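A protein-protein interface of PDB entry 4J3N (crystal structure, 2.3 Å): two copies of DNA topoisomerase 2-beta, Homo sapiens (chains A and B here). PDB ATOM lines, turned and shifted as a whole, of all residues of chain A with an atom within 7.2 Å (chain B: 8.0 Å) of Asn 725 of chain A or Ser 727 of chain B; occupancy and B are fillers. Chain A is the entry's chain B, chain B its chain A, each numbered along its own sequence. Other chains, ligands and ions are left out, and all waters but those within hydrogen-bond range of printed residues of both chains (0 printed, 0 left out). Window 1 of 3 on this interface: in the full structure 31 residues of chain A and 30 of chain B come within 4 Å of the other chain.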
ATOM      1  N   ILE A 663      -5.014 -13.194  27.872  1.00  0.00           N
ATOM      2  CA  ILE A 663      -5.674 -12.560  26.738  1.00  0.00           C
ATOM      3  C   ILE A 663      -6.917 -13.336  26.331  1.00  0.00           C
ATOM      4  O   ILE A 663      -7.769 -12.813  25.603  1.00  0.00           O
ATOM      5  CB  ILE A 663      -4.726 -12.459  25.514  1.00  0.00           C
ATOM      6  CG1 ILE A 663      -4.231 -13.851  25.098  1.00  0.00           C
ATOM      7  CG2 ILE A 663      -3.551 -11.539  25.817  1.00  0.00           C
ATOM      8  CD1 ILE A 663      -3.297 -13.837  23.879  1.00  0.00           C
ATOM      9  N   ASP A 719       0.404   0.195  18.664  1.00  0.00           N
ATOM     10  CA  ASP A 719       0.418  -0.980  17.795  1.00  0.00           C
ATOM     11  C   ASP A 719       1.104  -2.180  18.467  1.00  0.00           C
ATOM     12  O   ASP A 719       2.321  -2.204  18.604  1.00  0.00           O
ATOM     13  CB  ASP A 719       1.121  -0.641  16.478  1.00  0.00           C
ATOM     14  CG  ASP A 719       0.982  -1.744  15.425  1.00  0.00           C
ATOM     15  OD1 ASP A 719       0.749  -2.917  15.795  1.00  0.00           O
ATOM     16  OD2 ASP A 719       1.108  -1.433  14.221  1.00  0.00           O
ATOM     17  N   PHE A 720       0.321  -3.177  18.872  1.00  0.00           N
ATOM     18  CA  PHE A 720       0.882  -4.341  19.550  1.00  0.00           C
ATOM     19  C   PHE A 720       0.877  -5.611  18.683  1.00  0.00           C
ATOM     20  O   PHE A 720       1.094  -6.727  19.186  1.00  0.00           O
ATOM     21  CB  PHE A 720       0.164  -4.580  20.881  1.00  0.00           C
ATOM     22  CG  PHE A 720       0.247  -3.413  21.837  1.00  0.00           C
ATOM     23  CD1 PHE A 720       1.469  -3.027  22.384  1.00  0.00           C
ATOM     24  CD2 PHE A 720      -0.896  -2.709  22.197  1.00  0.00           C
ATOM     25  CE1 PHE A 720       1.551  -1.960  23.263  1.00  0.00           C
ATOM     26  CE2 PHE A 720      -0.829  -1.635  23.085  1.00  0.00           C
ATOM     27  CZ  PHE A 720       0.396  -1.261  23.612  1.00  0.00           C
ATOM     28  N   ASN A 721       0.652  -5.443  17.380  1.00  0.00           N
ATOM     29  CA  ASN A 721       0.660  -6.586  16.454  1.00  0.00           C
ATOM     30  C   ASN A 721       1.934  -7.400  16.515  1.00  0.00           C
ATOM     31  O   ASN A 721       1.895  -8.615  16.369  1.00  0.00           O
ATOM     32  CB  ASN A 721       0.414  -6.143  15.013  1.00  0.00           C
ATOM     33  CG  ASN A 721      -1.006  -5.655  14.790  1.00  0.00           C
ATOM     34  OD1 ASN A 721      -1.225  -4.534  14.325  1.00  0.00           O
ATOM     35  ND2 ASN A 721      -1.979  -6.491  15.133  1.00  0.00           N
ATOM     36  N   TYR A 722       3.072  -6.739  16.726  1.00  0.00           N
ATOM     37  CA  TYR A 722       4.346  -7.453  16.754  1.00  0.00           C
ATOM     38  C   TYR A 722       4.358  -8.478  17.889  1.00  0.00           C
ATOM     39  O   TYR A 722       5.069  -9.484  17.831  1.00  0.00           O
ATOM     40  CB  TYR A 722       5.525  -6.479  16.883  1.00  0.00           C
ATOM     41  CG  TYR A 722       5.677  -5.810  18.246  1.00  0.00           C
ATOM     42  CD1 TYR A 722       4.863  -4.746  18.623  1.00  0.00           C
ATOM     43  CD2 TYR A 722       6.658  -6.228  19.139  1.00  0.00           C
ATOM     44  CE1 TYR A 722       5.020  -4.121  19.858  1.00  0.00           C
ATOM     45  CE2 TYR A 722       6.813  -5.611  20.377  1.00  0.00           C
ATOM     46  CZ  TYR A 722       5.995  -4.557  20.721  1.00  0.00           C
ATOM     47  OH  TYR A 722       6.153  -3.946  21.942  1.00  0.00           O
ATOM     48  N   ILE A 723       3.563  -8.218  18.922  1.00  0.00           N
ATOM     49  CA  ILE A 723       3.426  -9.156  20.025  1.00  0.00           C
ATOM     50  C   ILE A 723       2.340 -10.210  19.747  1.00  0.00           C
ATOM     51  O   ILE A 723       2.603 -11.415  19.788  1.00  0.00           O
ATOM     52  CB  ILE A 723       3.076  -8.414  21.321  1.00  0.00           C
ATOM     53  CG1 ILE A 723       4.190  -7.430  21.716  1.00  0.00           C
ATOM     54  CG2 ILE A 723       2.788  -9.402  22.430  1.00  0.00           C
ATOM     55  CD1 ILE A 723       3.779  -6.495  22.860  1.00  0.00           C
ATOM     56  N   LEU A 724       1.129  -9.743  19.450  1.00  0.00           N
ATOM     57  CA  LEU A 724      -0.041 -10.624  19.253  1.00  0.00           C
ATOM     58  C   LEU A 724      -0.049 -11.470  17.963  1.00  0.00           C
ATOM     59  O   LEU A 724      -0.751 -12.474  17.894  1.00  0.00           O
ATOM     60  CB  LEU A 724      -1.344  -9.821  19.364  1.00  0.00           C
ATOM     61  CG  LEU A 724      -1.499  -9.195  20.752  1.00  0.00           C
ATOM     62  CD1 LEU A 724      -2.803  -8.421  20.880  1.00  0.00           C
ATOM     63  CD2 LEU A 724      -1.415 -10.270  21.806  1.00  0.00           C
ATOM     64  N   ASN A 725       0.713 -11.057  16.952  1.00  0.00           N
ATOM     65  CA  ASN A 725       0.916 -11.859  15.748  1.00  0.00           C
ATOM     66  C   ASN A 725       1.864 -13.029  15.962  1.00  0.00           C
ATOM     67  O   ASN A 725       1.956 -13.902  15.113  1.00  0.00           O
ATOM     68  CB  ASN A 725       1.460 -11.017  14.594  1.00  0.00           C
ATOM     69  CG  ASN A 725       0.421 -10.103  14.001  1.00  0.00           C
ATOM     70  OD1 ASN A 725      -0.764 -10.258  14.253  1.00  0.00           O
ATOM     71  ND2 ASN A 725       0.863  -9.138  13.205  1.00  0.00           N
ATOM     72  N   MET A 726       2.587 -13.051  17.073  1.00  0.00           N
ATOM     73  CA  MET A 726       3.413 -14.218  17.357  1.00  0.00           C
ATOM     74  C   MET A 726       2.527 -15.454  17.432  1.00  0.00           C
ATOM     75  O   MET A 726       1.344 -15.376  17.778  1.00  0.00           O
ATOM     76  CB  MET A 726       4.194 -14.059  18.666  1.00  0.00           C
ATOM     77  CG  MET A 726       5.147 -12.865  18.697  1.00  0.00           C
ATOM     78  SD  MET A 726       5.902 -12.670  20.333  1.00  0.00           S
ATOM     79  CE  MET A 726       7.264 -13.816  20.146  1.00  0.00           C
ATOM     80  N   SER A 727       3.114 -16.597  17.116  1.00  0.00           N
ATOM     81  CA  SER A 727       2.379 -17.838  17.032  1.00  0.00           C
ATOM     82  C   SER A 727       2.222 -18.440  18.419  1.00  0.00           C
ATOM     83  O   SER A 727       3.019 -18.167  19.320  1.00  0.00           O
ATOM     84  CB  SER A 727       3.150 -18.814  16.157  1.00  0.00           C
ATOM     85  OG  SER A 727       4.362 -19.168  16.807  1.00  0.00           O
ATOM     86  N   LEU A 728       1.199 -19.274  18.589  1.00  0.00           N
ATOM     87  CA  LEU A 728       1.041 -20.024  19.835  1.00  0.00           C
ATOM     88  C   LEU A 728       2.294 -20.813  20.191  1.00  0.00           C
ATOM     89  O   LEU A 728       2.568 -21.028  21.360  1.00  0.00           O
ATOM     90  CB  LEU A 728      -0.167 -20.952  19.745  1.00  0.00           C
ATOM     91  CG  LEU A 728      -1.457 -20.150  19.604  1.00  0.00           C
ATOM     92  CD1 LEU A 728      -2.611 -21.069  19.228  1.00  0.00           C
ATOM     93  CD2 LEU A 728      -1.728 -19.406  20.908  1.00  0.00           C
ATOM     94  N   SER A 730       5.123 -19.859  20.365  1.00  0.00           N
ATOM     95  CA  SER A 730       5.966 -18.967  21.169  1.00  0.00           C
ATOM     96  C   SER A 730       5.854 -19.210  22.675  1.00  0.00           C
ATOM     97  O   SER A 730       6.747 -18.842  23.423  1.00  0.00           O
ATOM     98  CB  SER A 730       5.604 -17.506  20.889  1.00  0.00           C
ATOM     99  OG  SER A 730       5.670 -17.222  19.506  1.00  0.00           O
ATOM    100  N   ILE B 653      -8.962 -23.745  20.230  1.00  0.00           N
ATOM    101  CA  ILE B 653      -9.132 -22.390  20.743  1.00  0.00           C
ATOM    102  C   ILE B 653     -10.146 -22.340  21.894  1.00  0.00           C
ATOM    103  O   ILE B 653      -9.950 -21.607  22.857  1.00  0.00           O
ATOM    104  CB  ILE B 653      -9.511 -21.387  19.623  1.00  0.00           C
ATOM    105  CG1 ILE B 653      -8.350 -21.223  18.629  1.00  0.00           C
ATOM    106  CG2 ILE B 653      -9.887 -20.033  20.204  1.00  0.00           C
ATOM    107  CD1 ILE B 653      -7.072 -20.691  19.247  1.00  0.00           C
ATOM    108  N   TYR B 722      -0.747 -26.437  11.971  1.00  0.00           N
ATOM    109  CA  TYR B 722      -1.894 -25.641  11.545  1.00  0.00           C
ATOM    110  C   TYR B 722      -2.624 -25.020  12.735  1.00  0.00           C
ATOM    111  O   TYR B 722      -3.333 -24.011  12.600  1.00  0.00           O
ATOM    112  CB  TYR B 722      -2.866 -26.461  10.684  1.00  0.00           C
ATOM    113  CG  TYR B 722      -3.659 -27.532  11.419  1.00  0.00           C
ATOM    114  CD1 TYR B 722      -5.002 -27.345  11.727  1.00  0.00           C
ATOM    115  CD2 TYR B 722      -3.065 -28.732  11.783  1.00  0.00           C
ATOM    116  CE1 TYR B 722      -5.728 -28.327  12.384  1.00  0.00           C
ATOM    117  CE2 TYR B 722      -3.775 -29.712  12.442  1.00  0.00           C
ATOM    118  CZ  TYR B 722      -5.103 -29.511  12.736  1.00  0.00           C
ATOM    119  OH  TYR B 722      -5.795 -30.504  13.392  1.00  0.00           O
ATOM    120  N   ILE B 723      -2.463 -25.631  13.895  1.00  0.00           N
ATOM    121  CA  ILE B 723      -3.042 -25.095  15.135  1.00  0.00           C
ATOM    122  C   ILE B 723      -2.068 -24.126  15.809  1.00  0.00           C
ATOM    123  O   ILE B 723      -2.395 -22.972  16.065  1.00  0.00           O
ATOM    124  CB  ILE B 723      -3.391 -26.239  16.125  1.00  0.00           C
ATOM    125  CG1 ILE B 723      -4.354 -27.238  15.466  1.00  0.00           C
ATOM    126  CG2 ILE B 723      -3.970 -25.682  17.405  1.00  0.00           C
ATOM    127  CD1 ILE B 723      -4.494 -28.565  16.212  1.00  0.00           C
ATOM    128  N   LEU B 724      -0.858 -24.604  16.073  1.00  0.00           N
ATOM    129  CA  LEU B 724       0.125 -23.838  16.834  1.00  0.00           C
ATOM    130  C   LEU B 724       0.739 -22.631  16.093  1.00  0.00           C
ATOM    131  O   LEU B 724       1.289 -21.726  16.728  1.00  0.00           O
ATOM    132  CB  LEU B 724       1.208 -24.784  17.363  1.00  0.00           C
ATOM    133  CG  LEU B 724       0.581 -25.826  18.312  1.00  0.00           C
ATOM    134  CD1 LEU B 724       1.460 -27.044  18.498  1.00  0.00           C
ATOM    135  CD2 LEU B 724       0.222 -25.208  19.664  1.00  0.00           C
ATOM    136  N   ASN B 725       0.656 -22.621  14.763  1.00  0.00           N
ATOM    137  CA  ASN B 725       1.053 -21.447  13.983  1.00  0.00           C
ATOM    138  C   ASN B 725       0.008 -20.348  14.062  1.00  0.00           C
ATOM    139  O   ASN B 725       0.230 -19.252  13.565  1.00  0.00           O
ATOM    140  CB  ASN B 725       1.267 -21.769  12.497  1.00  0.00           C
ATOM    141  CG  ASN B 725       2.492 -22.627  12.241  1.00  0.00           C
ATOM    142  OD1 ASN B 725       3.323 -22.829  13.118  1.00  0.00           O
ATOM    143  ND2 ASN B 725       2.607 -23.132  11.016  1.00  0.00           N
ATOM    144  N   MET B 726      -1.153 -20.639  14.637  1.00  0.00           N
ATOM    145  CA  MET B 726      -2.143 -19.580  14.806  1.00  0.00           C
ATOM    146  C   MET B 726      -1.524 -18.486  15.674  1.00  0.00           C
ATOM    147  O   MET B 726      -0.734 -18.771  16.563  1.00  0.00           O
ATOM    148  CB  MET B 726      -3.456 -20.109  15.412  1.00  0.00           C
ATOM    149  CG  MET B 726      -4.312 -20.903  14.394  1.00  0.00           C
ATOM    150  SD  MET B 726      -5.956 -21.365  14.992  1.00  0.00           S
ATOM    151  CE  MET B 726      -5.508 -22.600  16.196  1.00  0.00           C
ATOM    152  N   SER B 727      -1.861 -17.236  15.394  1.00  0.00           N
ATOM    153  CA  SER B 727      -1.339 -16.134  16.177  1.00  0.00           C
ATOM    154  C   SER B 727      -2.042 -16.046  17.546  1.00  0.00           C
ATOM    155  O   SER B 727      -3.121 -16.608  17.748  1.00  0.00           O
ATOM    156  CB  SER B 727      -1.492 -14.827  15.402  1.00  0.00           C
ATOM    157  OG  SER B 727      -2.856 -14.457  15.342  1.00  0.00           O
ATOM    158  N   LEU B 728      -1.416 -15.335  18.481  1.00  0.00           N
ATOM    159  CA  LEU B 728      -1.980 -15.112  19.807  1.00  0.00           C
ATOM    160  C   LEU B 728      -3.308 -14.362  19.721  1.00  0.00           C
ATOM    161  O   LEU B 728      -4.188 -14.531  20.570  1.00  0.00           O
ATOM    162  CB  LEU B 728      -0.975 -14.360  20.686  1.00  0.00           C
ATOM    163  CG  LEU B 728       0.240 -15.208  21.071  1.00  0.00           C
ATOM    164  CD1 LEU B 728       1.369 -14.357  21.672  1.00  0.00           C
ATOM    165  CD2 LEU B 728      -0.167 -16.326  22.026  1.00  0.00           C
ATOM    166  N   TRP B 729      -3.454 -13.533  18.696  1.00  0.00           N
ATOM    167  CA  TRP B 729      -4.736 -12.886  18.427  1.00  0.00           C
ATOM    168  C   TRP B 729      -5.890 -13.894  18.411  1.00  0.00           C
ATOM    169  O   TRP B 729      -7.006 -13.564  18.798  1.00  0.00           O
ATOM    170  CB  TRP B 729      -4.710 -12.195  17.078  1.00  0.00           C
ATOM    171  CG  TRP B 729      -4.164 -10.805  17.059  1.00  0.00           C
ATOM    172  CD1 TRP B 729      -3.138 -10.342  16.283  1.00  0.00           C
ATOM    173  CD2 TRP B 729      -4.641  -9.678  17.807  1.00  0.00           C
ATOM    174  NE1 TRP B 729      -2.944  -9.003  16.507  1.00  0.00           N
ATOM    175  CE2 TRP B 729      -3.846  -8.571  17.444  1.00  0.00           C
ATOM    176  CE3 TRP B 729      -5.656  -9.501  18.756  1.00  0.00           C
ATOM    177  CZ2 TRP B 729      -4.031  -7.303  17.993  1.00  0.00           C
ATOM    178  CZ3 TRP B 729      -5.840  -8.243  19.300  1.00  0.00           C
ATOM    179  CH2 TRP B 729      -5.031  -7.159  18.916  1.00  0.00           C
ATOM    180  N   SER B 730      -5.612 -15.109  17.944  1.00  0.00           N
ATOM    181  CA  SER B 730      -6.621 -16.173  17.850  1.00  0.00           C
ATOM    182  C   SER B 730      -7.368 -16.420  19.158  1.00  0.00           C
ATOM    183  O   SER B 730      -8.498 -16.896  19.131  1.00  0.00           O
ATOM    184  CB  SER B 730      -5.978 -17.496  17.414  1.00  0.00           C
ATOM    185  OG  SER B 730      -5.343 -17.362  16.161  1.00  0.00           O
ATOM    186  N   LEU B 731      -6.727 -16.119  20.287  1.00  0.00           N
ATOM    187  CA  LEU B 731      -7.306 -16.340  21.619  1.00  0.00           C
ATOM    188  C   LEU B 731      -8.234 -15.222  22.053  1.00  0.00           C
ATOM    189  O   LEU B 731      -8.928 -15.361  23.052  1.00  0.00           O
ATOM    190  CB  LEU B 731      -6.208 -16.498  22.675  1.00  0.00           C
ATOM    191  CG  LEU B 731      -5.174 -17.592  22.425  1.00  0.00           C
ATOM    192  CD1 LEU B 731      -4.047 -17.498  23.432  1.00  0.00           C
ATOM    193  CD2 LEU B 731      -5.800 -18.967  22.468  1.00  0.00           C
ATOM    194  N   THR B 732      -8.240 -14.111  21.316  1.00  0.00           N
ATOM    195  CA  THR B 732      -9.082 -12.975  21.686  1.00  0.00           C
ATOM    196  C   THR B 732     -10.534 -13.108  21.231  1.00  0.00           C
ATOM    197  O   THR B 732     -10.852 -13.903  20.344  1.00  0.00           O
ATOM    198  CB  THR B 732      -8.520 -11.628  21.183  1.00  0.00           C
ATOM    199  OG1 THR B 732      -8.621 -11.555  19.758  1.00  0.00           O
ATOM    200  CG2 THR B 732      -7.071 -11.455  21.616  1.00  0.00           C
ATOM    201  N   LYS B 735     -11.791 -12.806  17.573  1.00  0.00           N
ATOM    202  CA  LYS B 735     -11.187 -13.866  16.773  1.00  0.00           C
ATOM    203  C   LYS B 735     -11.802 -15.226  17.054  1.00  0.00           C
ATOM    204  O   LYS B 735     -11.940 -16.048  16.155  1.00  0.00           O
ATOM    205  CB  LYS B 735      -9.668 -13.916  16.978  1.00  0.00           C
ATOM    206  CG  LYS B 735      -8.977 -12.704  16.412  1.00  0.00           C
ATOM    207  CD  LYS B 735      -9.173 -12.652  14.929  1.00  0.00           C
ATOM    208  CE  LYS B 735      -8.370 -11.538  14.298  1.00  0.00           C
ATOM    209  NZ  LYS B 735      -8.515 -11.568  12.809  1.00  0.00           N
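Among the printed residues, pairs that only touch across the chains: Ile 663 of chain A with Leu 728 of chain B, Ile 663 of chain A with Leu 731 of chain B, Ile 723 of chain A with Leu 728 of chain B, Leu 724 of chain A with Ser 727 of chain B, Asn 725 of chain A with Ser 727 of chain B, Met 726 of chain A with Ser 727 of chain B, Ser 727 of chain A with Leu 724 of chain B, Ser 727 of chain A with Asn 725 of chain B, Ser 727 of chain A with Met 726 of chain B, Leu 728 of chain A with Ile 723 of chain B, Leu 728 of chain A with Leu 728 of chain B and Leu 728 of chain A with Leu 731 of chain B.
Hydrophobic or aromatic side chains of chain B within 4 Å of the printed part of chain A: Leu 728, Trp 729 and Leu 731. Of the 12 printed residues of chain A, 8 touch a printed residue of chain B. Hydrophobic or aromatic side chains of chain A that line the printed part of chain B: Ile 663, Leu 724 and Leu 728. Along chain A the printed residues that touch a printed residue of chain B span positions 663 to 728. Among the printed residues, no Asp or Glu carboxylate lies within 4 Å of a Lys or Arg side-chain nitrogen of the other chain.
OG of Ser 730 of chain B sits at hydrogen-bond distance from O of Ser 727 of chain B (2.8 Å). The side-chain hydroxyl of Thr 732 of chain B lies within hydrogen-bond range of the backbone carbonyl oxygen of Trp 729 of chain B (2.8 Å). The side-chain carboxylate (OD1) of Asp 719 of chain A sits close to the side-chain amide oxygen (OD1) of Asn 721 of chain A (2.9 Å). O of Asn 721 of chain A lies close to ND2 of Asn 725 of chain A, 3.4 Å away. O of Ser 727 of chain A lies within hydrogen-bond range of OG of Ser 730 of chain A (2.8 Å).
The backbone carbonyl oxygen (O) of Leu 724 of chain B is in hydrogen-bond range of the backbone NH (N) of Leu 728 of chain A (3.1 Å). The backbone carbonyl oxygen of Met 726 of chain B sits at hydrogen-bond distance from the backbone NH of Leu 728 of chain A (2.8 Å). The backbone NH of Leu 728 of chain B sits at hydrogen-bond distance from the backbone carbonyl oxygen of Leu 724 of chain A. O of Met 726 of chain A sits at hydrogen-bond distance from N of Leu 728 of chain B (2.8 Å). The side-chain amide nitrogen (ND2) of Asn 721 of chain A lies close to the indole nitrogen (NE1) of Trp 729 of chain B. The backbone NH (N) of Trp 729 of chain B is in hydrogen-bond range of the backbone carbonyl oxygen (O) of Leu 724 of chain A, at 3.0 Å. NE1 of Trp 729 of chain B sits close to OD1 of Asn 725 of chain A.
Ile 723 of chain A touches Leu 728 of chain B, and with the chains exchanged Leu 728 of chain A touches Ile 723 of chain B. Asn 725 of chain A touches Ser 727 of chain B, and with the chains exchanged Ser 727 of chain A touches Asn 725 of chain B. Met 726 of chain A touches Ser 727 of chain B, and with the chains exchanged Ser 727 of chain A touches Met 726 of chain B. Met 726 of chain A touches Leu 728 of chain B, and with the chains exchanged Leu 728 of chain A touches Met 726 of chain B.
Ser 727 of chain B touches just these residues of chain A: Leu 724, Asn 725 and Met 726. Printed residues of chain A within 4 Å of Leu 728 of chain B: Ile 663, Ile 723, Leu 724, Met 726 and Leu 728. Of the printed residues of chain B, Leu 728 of chain A touches Ile 723 (3.7 Å), Leu 724 (3.1 Å), Met 726 (2.8 Å), Leu 728 (3.6 Å) and Leu 731 (3.9 Å). Tyr 722 of chain A touches none of the printed residues of chain B. Thr 732 of chain B touches none of the printed residues of chain A. The nearest residue of chain B that does not touch Asn 725 of chain A is Leu 728 of chain B (4.7 Å). The nearest residue of chain A that does not touch Ser 727 of chain B is Ser 727 of chain A (4.2 Å).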
